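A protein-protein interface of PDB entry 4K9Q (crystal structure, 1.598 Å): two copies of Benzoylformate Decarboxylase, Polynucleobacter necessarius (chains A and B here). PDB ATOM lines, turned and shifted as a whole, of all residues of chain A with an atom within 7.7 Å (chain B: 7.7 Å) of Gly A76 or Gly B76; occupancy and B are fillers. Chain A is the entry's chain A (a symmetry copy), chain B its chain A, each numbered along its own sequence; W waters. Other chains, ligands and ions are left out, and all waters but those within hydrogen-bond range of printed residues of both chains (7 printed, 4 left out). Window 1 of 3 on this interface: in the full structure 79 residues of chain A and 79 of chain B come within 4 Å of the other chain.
Ala A73 touches Gly B80 (O to CA, 3.9 Å). Ala A73 touches Leu B83 (N to CD1, 3.9 Å). O of Gly A76 touches CB of Met B79, 3.3 Å away. Asn A77 touches Gly B80. Gly B76 touches Met A79. Met A79 touches Met B79 (CG to CB, 3.97 Å). Gly A80 touches Asn B77 (N to N, 3.7 Å). Leu A83 touches Gly B72 (CD1 to C, 3.5 Å). CD1 of Leu A83 touches N of Ala B73, 3.9 Å away. Met B118 touches Met A118 (O to O, 3.8 Å).
Ala A73 touches Gly B80, and with the chains exchanged Gly A80 touches Ala B73. Gly A76 touches Met B79, and with the chains exchanged Met A79 touches Gly B76. Gly A76 touches Gly B80, and with the chains exchanged Gly A80 touches Gly B76. Asn A77 touches Gly B80, and with the chains exchanged Gly A80 touches Asn B77. Of the 17 pairs that touch across the chains among the printed residues, 17 have their exchanged pair printed and touching as well.
O of Gly B76 lies close to N of Gly A80. N of Gly B80 sits close to O of Gly A76 (3.4 Å). The indole nitrogen (NE1) of Trp A122 sits at hydrogen-bond distance from the side-chain sulfur (SD) of Met B118 (3.5 Å). SD of Met A118 lies within hydrogen-bond range of NE1 of Trp B122, at 3.5 Å. O of Gly A76 sits close to O of Gly B76.
The side-chain carboxylate of Glu B47 sits at hydrogen-bond distance from the side-chain amide nitrogen of Asn B77, 3.0 Å away. The side-chain carboxylate (OE1) of Glu A47 sits at hydrogen-bond distance from the side-chain amide nitrogen (ND2) of Asn A77 (3.0 Å).
Hydrophobic or aromatic side chains of chain A within 4 Å of the printed part of chain B: Met A79, Leu A83, Met A118 and Trp A122.
Gly A76 touches just these residues of chain B: Gly B76 (3.1 Å), Met B79 (3.3 Å) and Gly B80 (3.2 Å). Gly B76 touches just these residues of chain A: Gly A76, Met A79 and Gly A80. Printed residues of chain A within 4 Å of Asn B77: Gly A80. Of the printed residues of chain A, Gly B80 touches Ala A73 (3.9 Å), Gly A76 (3.2 Å) and Asn A77 (3.7 Å). Printed residues of chain A within 4 Å of Leu B83: Gly A72 (3.5 Å) and Ala A73 (3.9 Å). Printed residues of chain A within 4 Å of Trp B122: Met A118 (3.5 Å). The nearest residue of chain B that does not touch Gly A76 is Asn B77 (4.5 Å). The nearest printed residue of chain A that does not touch Ala B73 is Met A79 (5.8 Å).
Water W7 lies within hydrogen-bond range of O of Met A118 (2.6 Å) and O of Met B118 (2.6 Å). Water W1 bridges the backbone carbonyl oxygen of Met A118 and the backbone carbonyl oxygen of Met B118. Water W5 lies within hydrogen-bond range of OD1 of Asn B112 (2.8 Å), NE1 of Trp A122 (2.8 Å) and SD of Met B118 (3.4 Å). Water W4 lies within hydrogen-bond range of O of Asn A77 (2.8 Å), O of Asn B77 (2.8 Å), NE2 of Gln B46 (3.0 Å) and NE2 of Gln A46 (3.0 Å). Water W2 bridges the side-chain amide oxygen (OD1) of Asn A77 (2.9 Å) and the side-chain sulfur (SG) of Cys B81 (3.6 Å). Water W3 bridges the side-chain amide oxygen of Asn B77 (2.9 Å) and the side-chain sulfur of Cys A81 (3.6 Å).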
ATOM      1  N   GLN A  46      13.287  12.803  13.185  1.00  0.00           N
ATOM      2  CA  GLN A  46      13.090  11.393  13.524  1.00  0.00           C
ATOM      3  C   GLN A  46      14.459  10.712  13.503  1.00  0.00           C
ATOM      4  O   GLN A  46      15.348  11.133  12.758  1.00  0.00           O
ATOM      5  CB  GLN A  46      12.113  10.732  12.542  1.00  0.00           C
ATOM      6  CG  GLN A  46      11.397   9.499  13.093  1.00  0.00           C
ATOM      7  CD  GLN A  46      12.057   8.191  12.682  1.00  0.00           C
ATOM      8  OE1 GLN A  46      13.106   8.187  12.030  1.00  0.00           O
ATOM      9  NE2 GLN A  46      11.432   7.074  13.046  1.00  0.00           N
ATOM     10  N   GLU A  47      14.641   9.686  14.333  1.00  0.00           N
ATOM     11  CA  GLU A  47      15.978   9.180  14.604  1.00  0.00           C
ATOM     12  C   GLU A  47      16.645   8.399  13.470  1.00  0.00           C
ATOM     13  O   GLU A  47      17.867   8.326  13.412  1.00  0.00           O
ATOM     14  CB  GLU A  47      15.995   8.397  15.921  1.00  0.00           C
ATOM     15  CG  GLU A  47      15.662   9.260  17.137  1.00  0.00           C
ATOM     16  CD  GLU A  47      14.164   9.407  17.409  1.00  0.00           C
ATOM     17  OE1 GLU A  47      13.332   8.990  16.565  1.00  0.00           O
ATOM     18  OE2 GLU A  47      13.828   9.956  18.485  1.00  0.00           O
ATOM     19  N   ALA A  48      15.865   7.818  12.561  1.00  0.00           N
ATOM     20  CA  ALA A  48      16.476   7.208  11.386  1.00  0.00           C
ATOM     21  C   ALA A  48      17.222   8.295  10.609  1.00  0.00           C
ATOM     22  O   ALA A  48      18.342   8.077  10.138  1.00  0.00           O
ATOM     23  CB  ALA A  48      15.424   6.528  10.506  1.00  0.00           C
ATOM     24  N   ILE A  69      20.555  10.788  20.791  1.00  0.00           N
ATOM     25  CA  ILE A  69      19.139  10.468  20.701  1.00  0.00           C
ATOM     26  C   ILE A  69      18.564  10.069  22.052  1.00  0.00           C
ATOM     27  O   ILE A  69      19.296   9.939  23.042  1.00  0.00           O
ATOM     28  CB  ILE A  69      18.870   9.405  19.620  1.00  0.00           C
ATOM     29  CG1 ILE A  69      19.631   8.107  19.927  1.00  0.00           C
ATOM     30  CG2 ILE A  69      19.245   9.947  18.234  1.00  0.00           C
ATOM     31  CD1 ILE A  69      19.597   7.113  18.764  1.00  0.00           C
ATOM     32  N   HIS A  70      17.250   9.885  22.090  1.00  0.00           N
ATOM     33  CA  HIS A  70      16.535   9.846  23.357  1.00  0.00           C
ATOM     34  C   HIS A  70      16.277   8.427  23.837  1.00  0.00           C
ATOM     35  O   HIS A  70      15.313   7.795  23.422  1.00  0.00           O
ATOM     36  CB  HIS A  70      15.204  10.578  23.230  1.00  0.00           C
ATOM     37  CG  HIS A  70      14.388  10.570  24.488  1.00  0.00           C
ATOM     38  ND1 HIS A  70      14.858  11.069  25.685  1.00  0.00           N
ATOM     39  CD2 HIS A  70      13.130  10.131  24.728  1.00  0.00           C
ATOM     40  CE1 HIS A  70      13.919  10.943  26.608  1.00  0.00           C
ATOM     41  NE2 HIS A  70      12.858  10.386  26.049  1.00  0.00           N
ATOM     42  N   THR A  71      17.131   7.961  24.742  1.00  0.00           N
ATOM     43  CA  THR A  71      16.962   6.674  25.414  1.00  0.00           C
ATOM     44  C   THR A  71      16.574   5.520  24.460  1.00  0.00           C
ATOM     45  O   THR A  71      17.012   5.496  23.304  1.00  0.00           O
ATOM     46  CB  THR A  71      16.065   6.834  26.683  1.00  0.00           C
ATOM     47  OG1 THR A  71      16.046   5.616  27.442  1.00  0.00           O
ATOM     48  CG2 THR A  71      14.632   7.273  26.340  1.00  0.00           C
ATOM     49  N   GLY A  72      15.821   4.539  24.943  1.00  0.00           N
ATOM     50  CA  GLY A  72      15.504   3.365  24.139  1.00  0.00           C
ATOM     51  C   GLY A  72      14.558   3.684  22.996  1.00  0.00           C
ATOM     52  O   GLY A  72      14.603   3.044  21.942  1.00  0.00           O
ATOM     53  N   ALA A  73      13.691   4.671  23.205  1.00  0.00           N
ATOM     54  CA  ALA A  73      12.700   5.062  22.193  1.00  0.00           C
ATOM     55  C   ALA A  73      13.391   5.577  20.940  1.00  0.00           C
ATOM     56  O   ALA A  73      13.070   5.178  19.818  1.00  0.00           O
ATOM     57  CB  ALA A  73      11.766   6.141  22.741  1.00  0.00           C
ATOM     58  N   GLY A  74      14.337   6.481  21.147  1.00  0.00           N
ATOM     59  CA  GLY A  74      15.086   7.074  20.062  1.00  0.00           C
ATOM     60  C   GLY A  74      16.014   6.064  19.427  1.00  0.00           C
ATOM     61  O   GLY A  74      16.098   5.966  18.196  1.00  0.00           O
ATOM     62  N   LEU A  75      16.726   5.306  20.256  1.00  0.00           N
ATOM     63  CA  LEU A  75      17.608   4.275  19.714  1.00  0.00           C
ATOM     64  C   LEU A  75      16.818   3.282  18.862  1.00  0.00           C
ATOM     65  O   LEU A  75      17.266   2.892  17.789  1.00  0.00           O
ATOM     66  CB  LEU A  75      18.373   3.568  20.827  1.00  0.00           C
ATOM     67  CG  LEU A  75      19.301   2.451  20.352  1.00  0.00           C
ATOM     68  CD1 LEU A  75      20.410   3.003  19.464  1.00  0.00           C
ATOM     69  CD2 LEU A  75      19.877   1.737  21.565  1.00  0.00           C
ATOM     70  N   GLY A  76      15.635   2.895  19.328  1.00  0.00           N
ATOM     71  CA  GLY A  76      14.780   1.994  18.568  1.00  0.00           C
ATOM     72  C   GLY A  76      14.448   2.521  17.179  1.00  0.00           C
ATOM     73  O   GLY A  76      14.605   1.810  16.187  1.00  0.00           O
ATOM     74  N   ASN A  77      13.988   3.767  17.101  1.00  0.00           N
ATOM     75  CA  ASN A  77      13.665   4.365  15.804  1.00  0.00           C
ATOM     76  C   ASN A  77      14.868   4.394  14.865  1.00  0.00           C
ATOM     77  O   ASN A  77      14.713   4.440  13.632  1.00  0.00           O
ATOM     78  CB  ASN A  77      13.119   5.785  15.980  1.00  0.00           C
ATOM     79  CG  ASN A  77      11.668   5.805  16.424  1.00  0.00           C
ATOM     80  OD1 ASN A  77      11.001   4.768  16.446  1.00  0.00           O
ATOM     81  ND2 ASN A  77      11.168   6.988  16.770  1.00  0.00           N
ATOM     82  N   ALA A  78      16.065   4.412  15.452  1.00  0.00           N
ATOM     83  CA  ALA A  78      17.300   4.515  14.678  1.00  0.00           C
ATOM     84  C   ALA A  78      17.921   3.189  14.219  1.00  0.00           C
ATOM     85  O   ALA A  78      18.921   3.211  13.501  1.00  0.00           O
ATOM     86  CB  ALA A  78      18.343   5.310  15.467  1.00  0.00           C
ATOM     87  N   MET A  79      17.376   2.050  14.637  1.00  0.00           N
ATOM     88  CA  MET A  79      18.112   0.788  14.470  1.00  0.00           C
ATOM     89  C   MET A  79      18.363   0.352  13.017  1.00  0.00           C
ATOM     90  O   MET A  79      19.375  -0.313  12.728  1.00  0.00           O
ATOM     91  CB  MET A  79      17.481  -0.358  15.281  1.00  0.00           C
ATOM     92  CG  MET A  79      17.808  -0.319  16.759  1.00  0.00           C
ATOM     93  SD  MET A  79      19.579  -0.368  17.109  1.00  0.00           S
ATOM     94  CE  MET A  79      20.125  -1.792  16.169  1.00  0.00           C
ATOM     95  N   GLY A  80      17.448   0.693  12.111  1.00  0.00           N
ATOM     96  CA  GLY A  80      17.630   0.357  10.705  1.00  0.00           C
ATOM     97  C   GLY A  80      18.807   1.127  10.115  1.00  0.00           C
ATOM     98  O   GLY A  80      19.675   0.568   9.441  1.00  0.00           O
ATOM     99  N   CYS A  81      18.859   2.423  10.374  1.00  0.00           N
ATOM    100  CA  CYS A  81      19.984   3.201   9.891  1.00  0.00           C
ATOM    101  C   CYS A  81      21.288   2.874  10.632  1.00  0.00           C
ATOM    102  O   CYS A  81      22.363   3.033  10.078  1.00  0.00           O
ATOM    103  CB  CYS A  81      19.659   4.693   9.891  1.00  0.00           C
ATOM    104  SG  CYS A  81      18.585   5.094   8.482  1.00  0.00           S
ATOM    105  N   LEU A  82      21.195   2.385  11.862  1.00  0.00           N
ATOM    106  CA  LEU A  82      22.400   1.977  12.573  1.00  0.00           C
ATOM    107  C   LEU A  82      22.981   0.703  11.934  1.00  0.00           C
ATOM    108  O   LEU A  82      24.181   0.604  11.718  1.00  0.00           O
ATOM    109  CB  LEU A  82      22.104   1.780  14.059  1.00  0.00           C
ATOM    110  CG  LEU A  82      23.308   1.359  14.906  1.00  0.00           C
ATOM    111  CD1 LEU A  82      24.478   2.300  14.684  1.00  0.00           C
ATOM    112  CD2 LEU A  82      22.906   1.342  16.380  1.00  0.00           C
ATOM    113  N   LEU A  83      22.119  -0.262  11.611  1.00  0.00           N
ATOM    114  CA  LEU A  83      22.545  -1.429  10.844  1.00  0.00           C
ATOM    115  C   LEU A  83      23.301  -0.950   9.605  1.00  0.00           C
ATOM    116  O   LEU A  83      24.385  -1.438   9.285  1.00  0.00           O
ATOM    117  CB  LEU A  83      21.322  -2.277  10.457  1.00  0.00           C
ATOM    118  CG  LEU A  83      21.467  -3.583   9.667  1.00  0.00           C
ATOM    119  CD1 LEU A  83      20.196  -4.418   9.780  1.00  0.00           C
ATOM    120  CD2 LEU A  83      21.771  -3.309   8.199  1.00  0.00           C
ATOM    121  N   ASN A 112      16.187   3.019  29.457  1.00  0.00           N
ATOM    122  CA  ASN A 112      16.646   2.176  28.378  1.00  0.00           C
ATOM    123  C   ASN A 112      17.102   0.865  29.010  1.00  0.00           C
ATOM    124  O   ASN A 112      18.262   0.719  29.402  1.00  0.00           O
ATOM    125  CB  ASN A 112      17.778   2.865  27.619  1.00  0.00           C
ATOM    126  CG  ASN A 112      18.046   2.225  26.280  1.00  0.00           C
ATOM    127  OD1 ASN A 112      17.410   1.227  25.917  1.00  0.00           O
ATOM    128  ND2 ASN A 112      18.981   2.802  25.524  1.00  0.00           N
ATOM    129  N   MET A 118      20.446  -3.561  23.407  1.00  0.00           N
ATOM    130  CA  MET A 118      19.534  -3.108  22.360  1.00  0.00           C
ATOM    131  C   MET A 118      20.163  -2.961  20.957  1.00  0.00           C
ATOM    132  O   MET A 118      19.611  -3.473  19.992  1.00  0.00           O
ATOM    133  CB  MET A 118      18.810  -1.824  22.774  1.00  0.00           C
ATOM    134  CG  MET A 118      17.660  -1.499  21.827  1.00  0.00           C
ATOM    135  SD  MET A 118      16.631  -0.153  22.381  1.00  0.00           S
ATOM    136  CE  MET A 118      15.369  -0.184  21.089  1.00  0.00           C
ATOM    137  N   TRP A 122      24.624  -4.672  15.990  1.00  0.00           N
ATOM    138  CA  TRP A 122      25.004  -3.670  14.996  1.00  0.00           C
ATOM    139  C   TRP A 122      25.899  -2.537  15.492  1.00  0.00           C
ATOM    140  O   TRP A 122      25.881  -1.438  14.942  1.00  0.00           O
ATOM    141  CB  TRP A 122      23.755  -3.128  14.309  1.00  0.00           C
ATOM    142  CG  TRP A 122      22.992  -4.232  13.630  1.00  0.00           C
ATOM    143  CD1 TRP A 122      21.786  -4.750  14.000  1.00  0.00           C
ATOM    144  CD2 TRP A 122      23.414  -4.971  12.480  1.00  0.00           C
ATOM    145  NE1 TRP A 122      21.419  -5.756  13.135  1.00  0.00           N
ATOM    146  CE2 TRP A 122      22.405  -5.915  12.197  1.00  0.00           C
ATOM    147  CE3 TRP A 122      24.550  -4.927  11.663  1.00  0.00           C
ATOM    148  CZ2 TRP A 122      22.487  -6.798  11.114  1.00  0.00           C
ATOM    149  CZ3 TRP A 122      24.637  -5.809  10.595  1.00  0.00           C
ATOM    150  CH2 TRP A 122      23.607  -6.726  10.328  1.00  0.00           C
ATOM    151  N   GLN B  46       6.267   2.747   6.304  1.00  0.00           N
ATOM    152  CA  GLN B  46       7.497   2.665   7.092  1.00  0.00           C
ATOM    153  C   GLN B  46       7.217   1.772   8.301  1.00  0.00           C
ATOM    154  O   GLN B  46       6.080   1.710   8.775  1.00  0.00           O
ATOM    155  CB  GLN B  46       7.962   4.065   7.517  1.00  0.00           C
ATOM    156  CG  GLN B  46       9.458   4.172   7.815  1.00  0.00           C
ATOM    157  CD  GLN B  46       9.781   4.060   9.298  1.00  0.00           C
ATOM    158  OE1 GLN B  46       8.892   3.832  10.125  1.00  0.00           O
ATOM    159  NE2 GLN B  46      11.053   4.241   9.641  1.00  0.00           N
ATOM    160  N   GLU B  47       8.237   1.062   8.782  1.00  0.00           N
ATOM    161  CA  GLU B  47       8.005  -0.029   9.717  1.00  0.00           C
ATOM    162  C   GLU B  47       7.600   0.375  11.136  1.00  0.00           C
ATOM    163  O   GLU B  47       6.968  -0.406  11.838  1.00  0.00           O
ATOM    164  CB  GLU B  47       9.197  -0.992   9.719  1.00  0.00           C
ATOM    165  CG  GLU B  47       9.411  -1.684   8.373  1.00  0.00           C
ATOM    166  CD  GLU B  47      10.248  -0.876   7.380  1.00  0.00           C
ATOM    167  OE1 GLU B  47      10.542   0.319   7.637  1.00  0.00           O
ATOM    168  OE2 GLU B  47      10.605  -1.455   6.326  1.00  0.00           O
ATOM    169  N   ALA B  48       7.943   1.586  11.569  1.00  0.00           N
ATOM    170  CA  ALA B  48       7.431   2.053  12.852  1.00  0.00           C
ATOM    171  C   ALA B  48       5.903   2.096  12.776  1.00  0.00           C
ATOM    172  O   ALA B  48       5.214   1.692  13.717  1.00  0.00           O
ATOM    173  CB  ALA B  48       8.001   3.429  13.206  1.00  0.00           C
ATOM    174  N   ILE B  69       7.638  -7.719   8.122  1.00  0.00           N
ATOM    175  CA  ILE B  69       8.562  -6.688   7.675  1.00  0.00           C
ATOM    176  C   ILE B  69       9.828  -7.286   7.077  1.00  0.00           C
ATOM    177  O   ILE B  69      10.030  -8.506   7.107  1.00  0.00           O
ATOM    178  CB  ILE B  69       8.872  -5.684   8.801  1.00  0.00           C
ATOM    179  CG1 ILE B  69       9.501  -6.393  10.009  1.00  0.00           C
ATOM    180  CG2 ILE B  69       7.600  -4.929   9.208  1.00  0.00           C
ATOM    181  CD1 ILE B  69       9.597  -5.490  11.241  1.00  0.00           C
ATOM    182  N   HIS B  70      10.670  -6.422   6.525  1.00  0.00           N
ATOM    183  CA  HIS B  70      11.724  -6.872   5.627  1.00  0.00           C
ATOM    184  C   HIS B  70      13.064  -7.016   6.328  1.00  0.00           C
ATOM    185  O   HIS B  70      13.793  -6.045   6.486  1.00  0.00           O
ATOM    186  CB  HIS B  70      11.873  -5.896   4.466  1.00  0.00           C
ATOM    187  CG  HIS B  70      12.954  -6.272   3.497  1.00  0.00           C
ATOM    188  ND1 HIS B  70      12.978  -7.483   2.837  1.00  0.00           N
ATOM    189  CD2 HIS B  70      14.042  -5.588   3.072  1.00  0.00           C
ATOM    190  CE1 HIS B  70      14.033  -7.526   2.043  1.00  0.00           C
ATOM    191  NE2 HIS B  70      14.689  -6.384   2.160  1.00  0.00           N
ATOM    192  N   THR B  71      13.386  -8.249   6.706  1.00  0.00           N
ATOM    193  CA  THR B  71      14.688  -8.600   7.270  1.00  0.00           C
ATOM    194  C   THR B  71      15.188  -7.606   8.346  1.00  0.00           C
ATOM    195  O   THR B  71      14.381  -7.049   9.100  1.00  0.00           O
ATOM    196  CB  THR B  71      15.705  -8.932   6.132  1.00  0.00           C
ATOM    197  OG1 THR B  71      16.925  -9.449   6.683  1.00  0.00           O
ATOM    198  CG2 THR B  71      15.996  -7.722   5.229  1.00  0.00           C
ATOM    199  N   GLY B  72      16.498  -7.430   8.470  1.00  0.00           N
ATOM    200  CA  GLY B  72      17.050  -6.595   9.531  1.00  0.00           C
ATOM    201  C   GLY B  72      16.755  -5.121   9.320  1.00  0.00           C
ATOM    202  O   GLY B  72      16.625  -4.359  10.281  1.00  0.00           O
ATOM    203  N   ALA B  73      16.656  -4.713   8.057  1.00  0.00           N
ATOM    204  CA  ALA B  73      16.404  -3.307   7.712  1.00  0.00           C
ATOM    205  C   ALA B  73      15.049  -2.864   8.242  1.00  0.00           C
ATOM    206  O   ALA B  73      14.917  -1.811   8.870  1.00  0.00           O
ATOM    207  CB  ALA B  73      16.451  -3.106   6.199  1.00  0.00           C
ATOM    208  N   GLY B  74      14.040  -3.677   7.966  1.00  0.00           N
ATOM    209  CA  GLY B  74      12.687  -3.397   8.392  1.00  0.00           C
ATOM    210  C   GLY B  74      12.551  -3.532   9.892  1.00  0.00           C
ATOM    211  O   GLY B  74      11.945  -2.680  10.554  1.00  0.00           O
ATOM    212  N   LEU B  75      13.108  -4.606  10.446  1.00  0.00           N
ATOM    213  CA  LEU B  75      13.058  -4.778  11.896  1.00  0.00           C
ATOM    214  C   LEU B  75      13.715  -3.592  12.602  1.00  0.00           C
ATOM    215  O   LEU B  75      13.192  -3.095  13.595  1.00  0.00           O
ATOM    216  CB  LEU B  75      13.696  -6.098  12.314  1.00  0.00           C
ATOM    217  CG  LEU B  75      13.714  -6.347  13.821  1.00  0.00           C
ATOM    218  CD1 LEU B  75      12.298  -6.456  14.373  1.00  0.00           C
ATOM    219  CD2 LEU B  75      14.509  -7.613  14.103  1.00  0.00           C
ATOM    220  N   GLY B  76      14.844  -3.127  12.078  1.00  0.00           N
ATOM    221  CA  GLY B  76      15.520  -1.968  12.642  1.00  0.00           C
ATOM    222  C   GLY B  76      14.632  -0.733  12.701  1.00  0.00           C
ATOM    223  O   GLY B  76      14.523  -0.090  13.745  1.00  0.00           O
ATOM    224  N   ASN B  77      13.995  -0.394  11.583  1.00  0.00           N
ATOM    225  CA  ASN B  77      13.102   0.765  11.553  1.00  0.00           C
ATOM    226  C   ASN B  77      11.963   0.643  12.561  1.00  0.00           C
ATOM    227  O   ASN B  77      11.386   1.656  12.996  1.00  0.00           O
ATOM    228  CB  ASN B  77      12.522   0.970  10.150  1.00  0.00           C
ATOM    229  CG  ASN B  77      13.508   1.623   9.198  1.00  0.00           C
ATOM    230  OD1 ASN B  77      14.575   2.082   9.612  1.00  0.00           O
ATOM    231  ND2 ASN B  77      13.152   1.677   7.918  1.00  0.00           N
ATOM    232  N   ALA B  78      11.613  -0.598  12.898  1.00  0.00           N
ATOM    233  CA  ALA B  78      10.491  -0.864  13.796  1.00  0.00           C
ATOM    234  C   ALA B  78      10.822  -0.913  15.293  1.00  0.00           C
ATOM    235  O   ALA B  78       9.909  -1.061  16.106  1.00  0.00           O
ATOM    236  CB  ALA B  78       9.801  -2.170  13.392  1.00  0.00           C
ATOM    237  N   MET B  79      12.095  -0.826  15.670  1.00  0.00           N
ATOM    238  CA  MET B  79      12.470  -1.170  17.049  1.00  0.00           C
ATOM    239  C   MET B  79      11.890  -0.259  18.143  1.00  0.00           C
ATOM    240  O   MET B  79      11.653  -0.713  19.277  1.00  0.00           O
ATOM    241  CB  MET B  79      13.994  -1.314  17.212  1.00  0.00           C
ATOM    242  CG  MET B  79      14.547  -2.625  16.694  1.00  0.00           C
ATOM    243  SD  MET B  79      13.817  -4.078  17.478  1.00  0.00           S
ATOM    244  CE  MET B  79      14.008  -3.720  19.223  1.00  0.00           C
ATOM    245  N   GLY B  80      11.684   1.019  17.826  1.00  0.00           N
ATOM    246  CA  GLY B  80      11.098   1.940  18.791  1.00  0.00           C
ATOM    247  C   GLY B  80       9.650   1.561  19.086  1.00  0.00           C
ATOM    248  O   GLY B  80       9.222   1.485  20.239  1.00  0.00           O
ATOM    249  N   CYS B  81       8.879   1.305  18.042  1.00  0.00           N
ATOM    250  CA  CYS B  81       7.508   0.881  18.257  1.00  0.00           C
ATOM    251  C   CYS B  81       7.413  -0.538  18.835  1.00  0.00           C
ATOM    252  O   CYS B  81       6.450  -0.860  19.511  1.00  0.00           O
ATOM    253  CB  CYS B  81       6.673   1.065  16.991  1.00  0.00           C
ATOM    254  SG  CYS B  81       6.255   2.819  16.773  1.00  0.00           S
ATOM    255  N   LEU B  82       8.420  -1.370  18.601  1.00  0.00           N
ATOM    256  CA  LEU B  82       8.417  -2.698  19.201  1.00  0.00           C
ATOM    257  C   LEU B  82       8.642  -2.589  20.721  1.00  0.00           C
ATOM    258  O   LEU B  82       7.960  -3.238  21.501  1.00  0.00           O
ATOM    259  CB  LEU B  82       9.465  -3.589  18.536  1.00  0.00           C
ATOM    260  CG  LEU B  82       9.541  -5.015  19.085  1.00  0.00           C
ATOM    261  CD1 LEU B  82       8.169  -5.665  19.087  1.00  0.00           C
ATOM    262  CD2 LEU B  82      10.518  -5.830  18.239  1.00  0.00           C
ATOM    263  N   LEU B  83       9.589  -1.745  21.135  1.00  0.00           N
ATOM    264  CA  LEU B  83       9.759  -1.440  22.552  1.00  0.00           C
ATOM    265  C   LEU B  83       8.400  -1.049  23.135  1.00  0.00           C
ATOM    266  O   LEU B  83       7.990  -1.534  24.189  1.00  0.00           O
ATOM    267  CB  LEU B  83      10.785  -0.308  22.725  1.00  0.00           C
ATOM    268  CG  LEU B  83      11.187   0.208  24.112  1.00  0.00           C
ATOM    269  CD1 LEU B  83      12.486   1.003  24.029  1.00  0.00           C
ATOM    270  CD2 LEU B  83      10.092   1.078  24.716  1.00  0.00           C
ATOM    271  N   ASN B 112      19.633 -10.967   7.774  1.00  0.00           N
ATOM    272  CA  ASN B 112      19.407 -10.461   9.108  1.00  0.00           C
ATOM    273  C   ASN B 112      20.373 -11.204  10.026  1.00  0.00           C
ATOM    274  O   ASN B 112      20.054 -12.273  10.552  1.00  0.00           O
ATOM    275  CB  ASN B 112      17.952 -10.684   9.515  1.00  0.00           C
ATOM    276  CG  ASN B 112      17.559  -9.863  10.718  1.00  0.00           C
ATOM    277  OD1 ASN B 112      18.386  -9.142  11.290  1.00  0.00           O
ATOM    278  ND2 ASN B 112      16.285  -9.952  11.104  1.00  0.00           N
ATOM    279  N   MET B 118      18.725  -9.228  17.479  1.00  0.00           N
ATOM    280  CA  MET B 118      18.369  -7.851  17.145  1.00  0.00           C
ATOM    281  C   MET B 118      17.221  -7.246  17.980  1.00  0.00           C
ATOM    282  O   MET B 118      17.368  -6.149  18.504  1.00  0.00           O
ATOM    283  CB  MET B 118      18.099  -7.698  15.646  1.00  0.00           C
ATOM    284  CG  MET B 118      18.009  -6.231  15.240  1.00  0.00           C
ATOM    285  SD  MET B 118      17.930  -5.976  13.477  1.00  0.00           S
ATOM    286  CE  MET B 118      17.964  -4.171  13.430  1.00  0.00           C
ATOM    287  N   TRP B 122      13.467  -6.558  23.720  1.00  0.00           N
ATOM    288  CA  TRP B 122      12.082  -6.107  23.616  1.00  0.00           C
ATOM    289  C   TRP B 122      11.093  -7.104  23.018  1.00  0.00           C
ATOM    290  O   TRP B 122      10.079  -6.713  22.443  1.00  0.00           O
ATOM    291  CB  TRP B 122      12.030  -4.770  22.885  1.00  0.00           C
ATOM    292  CG  TRP B 122      12.835  -3.728  23.610  1.00  0.00           C
ATOM    293  CD1 TRP B 122      14.017  -3.173  23.212  1.00  0.00           C
ATOM    294  CD2 TRP B 122      12.523  -3.147  24.880  1.00  0.00           C
ATOM    295  NE1 TRP B 122      14.450  -2.263  24.150  1.00  0.00           N
ATOM    296  CE2 TRP B 122      13.554  -2.234  25.187  1.00  0.00           C
ATOM    297  CE3 TRP B 122      11.472  -3.314  25.789  1.00  0.00           C
ATOM    298  CZ2 TRP B 122      13.555  -1.470  26.359  1.00  0.00           C
ATOM    299  CZ3 TRP B 122      11.477  -2.565  26.957  1.00  0.00           C
ATOM    300  CH2 TRP B 122      12.508  -1.650  27.226  1.00  0.00           C
HETATM  301  O   HOH W   1      17.533  -3.429  18.204  1.00  0.00           O
HETATM  302  O   HOH W   2       8.335   5.732  16.800  1.00  0.00           O
HETATM  303  O   HOH W   3      15.524   3.599   7.384  1.00  0.00           O
HETATM  304  O   HOH W   4      12.187   4.294  12.373  1.00  0.00           O
HETATM  305  O   HOH W   5      20.294  -8.349  13.109  1.00  0.00           O
HETATM  306  O   HOH W   6      16.788  -1.422  25.499  1.00  0.00           O
HETATM  307  O   HOH W   7      19.331  -6.027  20.166  1.00  0.00           O
